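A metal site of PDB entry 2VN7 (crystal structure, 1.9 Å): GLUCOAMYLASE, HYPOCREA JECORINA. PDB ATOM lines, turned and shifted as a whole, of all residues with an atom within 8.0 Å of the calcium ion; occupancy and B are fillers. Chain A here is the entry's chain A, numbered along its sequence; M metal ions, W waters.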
ATOM      1  N   VAL A 181      17.248 -30.407   6.597  1.00  0.00           N
ATOM      2  CA  VAL A 181      16.698 -29.057   6.642  1.00  0.00           C
ATOM      3  C   VAL A 181      17.456 -28.115   5.700  1.00  0.00           C
ATOM      4  O   VAL A 181      18.656 -27.894   5.874  1.00  0.00           O
ATOM      5  CB  VAL A 181      16.646 -28.506   8.107  1.00  0.00           C
ATOM      6  CG1 VAL A 181      16.127 -27.083   8.138  1.00  0.00           C
ATOM      7  CG2 VAL A 181      15.766 -29.394   8.955  1.00  0.00           C
ATOM      8  N   SER A 184      19.714 -22.139   6.771  1.00  0.00           N
ATOM      9  CA  SER A 184      20.986 -21.693   7.348  1.00  0.00           C
ATOM     10  C   SER A 184      21.139 -22.449   8.645  1.00  0.00           C
ATOM     11  O   SER A 184      20.240 -22.446   9.473  1.00  0.00           O
ATOM     12  CB  SER A 184      21.001 -20.182   7.594  1.00  0.00           C
ATOM     13  OG  SER A 184      20.917 -19.446   6.368  1.00  0.00           O
ATOM     14  N   PHE A 227      21.216 -16.864  15.313  1.00  0.00           N
ATOM     15  CA  PHE A 227      20.674 -18.175  15.660  1.00  0.00           C
ATOM     16  C   PHE A 227      20.190 -18.227  17.135  1.00  0.00           C
ATOM     17  O   PHE A 227      19.339 -19.057  17.482  1.00  0.00           O
ATOM     18  CB  PHE A 227      21.732 -19.260  15.430  1.00  0.00           C
ATOM     19  CG  PHE A 227      22.053 -19.512  13.972  1.00  0.00           C
ATOM     20  CD1 PHE A 227      22.940 -18.683  13.271  1.00  0.00           C
ATOM     21  CD2 PHE A 227      21.469 -20.575  13.291  1.00  0.00           C
ATOM     22  CE1 PHE A 227      23.249 -18.923  11.920  1.00  0.00           C
ATOM     23  CE2 PHE A 227      21.774 -20.827  11.929  1.00  0.00           C
ATOM     24  CZ  PHE A 227      22.642 -19.992  11.254  1.00  0.00           C
ATOM     25  N   VAL A 229      18.214 -17.603  20.412  1.00  0.00           N
ATOM     26  CA  VAL A 229      16.855 -17.269  20.814  1.00  0.00           C
ATOM     27  C   VAL A 229      16.930 -16.747  22.261  1.00  0.00           C
ATOM     28  O   VAL A 229      17.001 -17.532  23.197  1.00  0.00           O
ATOM     29  CB  VAL A 229      15.926 -18.492  20.730  1.00  0.00           C
ATOM     30  CG1 VAL A 229      14.491 -18.107  21.118  1.00  0.00           C
ATOM     31  CG2 VAL A 229      15.970 -19.130  19.322  1.00  0.00           C
ATOM     32  N   TYR A 234      18.419 -20.443  24.146  1.00  0.00           N
ATOM     33  CA  TYR A 234      18.975 -21.555  23.393  1.00  0.00           C
ATOM     34  C   TYR A 234      19.258 -21.184  21.934  1.00  0.00           C
ATOM     35  O   TYR A 234      18.815 -20.141  21.467  1.00  0.00           O
ATOM     36  CB  TYR A 234      18.059 -22.784  23.483  1.00  0.00           C
ATOM     37  CG  TYR A 234      16.791 -22.664  22.651  1.00  0.00           C
ATOM     38  CD1 TYR A 234      15.660 -22.028  23.161  1.00  0.00           C
ATOM     39  CD2 TYR A 234      16.740 -23.148  21.350  1.00  0.00           C
ATOM     40  CE1 TYR A 234      14.515 -21.886  22.406  1.00  0.00           C
ATOM     41  CE2 TYR A 234      15.583 -23.004  20.579  1.00  0.00           C
ATOM     42  CZ  TYR A 234      14.482 -22.377  21.116  1.00  0.00           C
ATOM     43  OH  TYR A 234      13.334 -22.256  20.360  1.00  0.00           O
ATOM     44  N   VAL A 235      19.966 -22.050  21.225  1.00  0.00           N
ATOM     45  CA  VAL A 235      20.249 -21.820  19.811  1.00  0.00           C
ATOM     46  C   VAL A 235      19.151 -22.484  18.969  1.00  0.00           C
ATOM     47  O   VAL A 235      18.833 -23.670  19.115  1.00  0.00           O
ATOM     48  CB  VAL A 235      21.651 -22.336  19.396  1.00  0.00           C
ATOM     49  CG1 VAL A 235      21.839 -22.281  17.881  1.00  0.00           C
ATOM     50  CG2 VAL A 235      22.753 -21.519  20.071  1.00  0.00           C
ATOM     51  N   ASP A 236      18.563 -21.688  18.086  1.00  0.00           N
ATOM     52  CA  ASP A 236      17.711 -22.261  17.047  1.00  0.00           C
ATOM     53  C   ASP A 236      18.654 -22.732  15.940  1.00  0.00           C
ATOM     54  O   ASP A 236      19.234 -21.909  15.231  1.00  0.00           O
ATOM     55  CB  ASP A 236      16.678 -21.251  16.544  1.00  0.00           C
ATOM     56  CG  ASP A 236      15.839 -21.805  15.389  1.00  0.00           C
ATOM     57  OD1 ASP A 236      16.035 -22.988  15.009  1.00  0.00           O
ATOM     58  OD2 ASP A 236      14.988 -21.056  14.865  1.00  0.00           O
ATOM     59  N   SER A 237      18.829 -24.041  15.830  1.00  0.00           N
ATOM     60  CA  SER A 237      19.930 -24.599  15.032  1.00  0.00           C
ATOM     61  C   SER A 237      19.802 -24.364  13.524  1.00  0.00           C
ATOM     62  O   SER A 237      20.816 -24.390  12.809  1.00  0.00           O
ATOM     63  CB  SER A 237      20.115 -26.095  15.296  1.00  0.00           C
ATOM     64  OG  SER A 237      20.574 -26.308  16.615  1.00  0.00           O
ATOM     65  N   ASN A 238      18.571 -24.151  13.067  1.00  0.00           N
ATOM     66  CA  ASN A 238      18.313 -23.839  11.658  1.00  0.00           C
ATOM     67  C   ASN A 238      17.359 -22.644  11.512  1.00  0.00           C
ATOM     68  O   ASN A 238      16.229 -22.667  12.032  1.00  0.00           O
ATOM     69  CB  ASN A 238      17.769 -25.049  10.908  1.00  0.00           C
ATOM     70  CG  ASN A 238      18.734 -26.250  10.924  1.00  0.00           C
ATOM     71  OD1 ASN A 238      18.620 -27.145  11.767  1.00  0.00           O
ATOM     72  ND2 ASN A 238      19.694 -26.250  10.017  1.00  0.00           N
ATOM     73  N   ILE A 239      17.835 -21.619  10.811  1.00  0.00           N
ATOM     74  CA  ILE A 239      17.075 -20.406  10.570  1.00  0.00           C
ATOM     75  C   ILE A 239      16.958 -20.208   9.038  1.00  0.00           C
ATOM     76  O   ILE A 239      17.377 -21.077   8.285  1.00  0.00           O
ATOM     77  CB  ILE A 239      17.685 -19.158  11.291  1.00  0.00           C
ATOM     78  CG1 ILE A 239      19.113 -18.855  10.816  1.00  0.00           C
ATOM     79  CG2 ILE A 239      17.632 -19.362  12.842  1.00  0.00           C
ATOM     80  CD1 ILE A 239      19.614 -17.490  11.223  1.00  0.00           C
ATOM     81  N   ASN A 240      16.379 -19.078   8.614  1.00  0.00           N
ATOM     82  CA  ASN A 240      16.076 -18.827   7.192  1.00  0.00           C
ATOM     83  C   ASN A 240      15.138 -19.874   6.574  1.00  0.00           C
ATOM     84  O   ASN A 240      15.063 -20.063   5.347  1.00  0.00           O
ATOM     85  CB  ASN A 240      17.360 -18.618   6.378  1.00  0.00           C
ATOM     86  CG  ASN A 240      17.968 -17.263   6.625  1.00  0.00           C
ATOM     87  OD1 ASN A 240      17.255 -16.312   6.993  1.00  0.00           O
ATOM     88  ND2 ASN A 240      19.265 -17.149   6.438  1.00  0.00           N
ATOM     89  N   THR A 241      14.399 -20.519   7.474  1.00  0.00           N
ATOM     90  CA  THR A 241      13.397 -21.520   7.149  1.00  0.00           C
ATOM     91  C   THR A 241      12.519 -21.737   8.377  1.00  0.00           C
ATOM     92  O   THR A 241      12.909 -21.391   9.489  1.00  0.00           O
ATOM     93  CB  THR A 241      14.021 -22.869   6.700  1.00  0.00           C
ATOM     94  OG1 THR A 241      12.977 -23.759   6.307  1.00  0.00           O
ATOM     95  CG2 THR A 241      14.855 -23.521   7.795  1.00  0.00           C
ATOM     96  N   ASN A 242      11.328 -22.279   8.173  1.00  0.00           N
ATOM     97  CA  ASN A 242      10.545 -22.780   9.292  1.00  0.00           C
ATOM     98  C   ASN A 242      10.450 -24.289   9.150  1.00  0.00           C
ATOM     99  O   ASN A 242       9.674 -24.805   8.345  1.00  0.00           O
ATOM    100  CB  ASN A 242       9.196 -22.066   9.424  1.00  0.00           C
ATOM    101  CG  ASN A 242       9.331 -20.554   9.576  1.00  0.00           C
ATOM    102  OD1 ASN A 242       9.737 -20.051  10.646  1.00  0.00           O
ATOM    103  ND2 ASN A 242       9.044 -19.823   8.514  1.00  0.00           N
ATOM    104  N   GLU A 243      11.290 -24.979   9.907  1.00  0.00           N
ATOM    105  CA  GLU A 243      11.460 -26.412   9.725  1.00  0.00           C
ATOM    106  C   GLU A 243      10.424 -27.242  10.504  1.00  0.00           C
ATOM    107  O   GLU A 243      10.434 -28.468  10.444  1.00  0.00           O
ATOM    108  CB  GLU A 243      12.921 -26.822  10.025  1.00  0.00           C
ATOM    109  CG  GLU A 243      13.311 -26.787  11.505  1.00  0.00           C
ATOM    110  CD  GLU A 243      13.677 -25.399  12.020  1.00  0.00           C
ATOM    111  OE1 GLU A 243      13.324 -24.342  11.407  1.00  0.00           O
ATOM    112  OE2 GLU A 243      14.340 -25.330  13.071  1.00  0.00           O
ATOM    113  N   GLY A 244       9.504 -26.569  11.191  1.00  0.00           N
ATOM    114  CA  GLY A 244       8.482 -27.249  11.990  1.00  0.00           C
ATOM    115  C   GLY A 244       9.044 -27.871  13.277  1.00  0.00           C
ATOM    116  O   GLY A 244       8.553 -28.903  13.755  1.00  0.00           O
ATOM    117  N   ARG A 245      10.089 -27.251  13.810  1.00  0.00           N
ATOM    118  CA  ARG A 245      10.744 -27.691  15.053  1.00  0.00           C
ATOM    119  C   ARG A 245      11.116 -26.484  15.909  1.00  0.00           C
ATOM    120  O   ARG A 245      11.107 -25.343  15.446  1.00  0.00           O
ATOM    121  CB  ARG A 245      12.021 -28.472  14.743  1.00  0.00           C
ATOM    122  CG  ARG A 245      11.882 -29.663  13.825  1.00  0.00           C
ATOM    123  CD  ARG A 245      13.257 -30.232  13.544  1.00  0.00           C
ATOM    124  NE  ARG A 245      13.314 -31.066  12.349  1.00  0.00           N
ATOM    125  CZ  ARG A 245      14.434 -31.478  11.773  1.00  0.00           C
ATOM    126  NH1 ARG A 245      15.625 -31.156  12.294  1.00  0.00           N
ATOM    127  NH2 ARG A 245      14.378 -32.242  10.688  1.00  0.00           N
ATOM    128  N   THR A 246      11.471 -26.737  17.173  1.00  0.00           N
ATOM    129  CA  THR A 246      11.953 -25.666  18.060  1.00  0.00           C
ATOM    130  C   THR A 246      13.360 -25.186  17.668  1.00  0.00           C
ATOM    131  O   THR A 246      13.763 -24.064  17.981  1.00  0.00           O
ATOM    132  CB  THR A 246      12.037 -26.164  19.507  1.00  0.00           C
ATOM    133  OG1 THR A 246      13.036 -27.195  19.567  1.00  0.00           O
ATOM    134  CG2 THR A 246      10.690 -26.726  19.982  1.00  0.00           C
ATOM    135  N   GLY A 247      14.131 -26.061  17.012  1.00  0.00           N
ATOM    136  CA  GLY A 247      15.527 -25.776  16.704  1.00  0.00           C
ATOM    137  C   GLY A 247      16.500 -26.208  17.814  1.00  0.00           C
ATOM    138  O   GLY A 247      17.705 -26.145  17.637  1.00  0.00           O
ATOM    139  N   LYS A 248      15.959 -26.654  18.942  1.00  0.00           N
ATOM    140  CA  LYS A 248      16.779 -27.353  19.969  1.00  0.00           C
ATOM    141  C   LYS A 248      17.298 -28.662  19.365  1.00  0.00           C
ATOM    142  O   LYS A 248      16.490 -29.543  19.054  1.00  0.00           O
ATOM    143  CB  LYS A 248      15.933 -27.642  21.215  1.00  0.00           C
ATOM    144  CG  LYS A 248      15.309 -26.414  21.822  1.00  0.00           C
ATOM    145  CD  LYS A 248      14.344 -26.794  22.969  1.00  0.00           C
ATOM    146  CE  LYS A 248      13.485 -25.580  23.345  1.00  0.00           C
ATOM    147  NZ  LYS A 248      12.409 -25.946  24.315  1.00  0.00           N
HETATM  148 CA    CA M   1      14.379 -22.951  13.301  1.00  0.00          CA
HETATM  149  O   HOH W   1      13.276 -21.243  12.144  1.00  0.00           O
HETATM  150  O   HOH W   2      12.418 -23.092  14.687  1.00  0.00           O
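The nearest printed residue that does not touch the calcium ion is Thr 241 (4.4 Å).
The calcium ion is bound by O of Asn 238 (2.3 Å), water W1 (2.3 Å), OD1 of Asp 236 (2.4 Å), OE2 of Glu 243 (2.4 Å), water W2 (2.4 Å), OD2 of Asp 236 (2.5 Å) and OE1 of Glu 243 (2.6 Å).
The backbone NH (N) of Asp 236 sits at hydrogen-bond distance from the backbone carbonyl oxygen (O) of Phe 227, at 2.8 Å.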
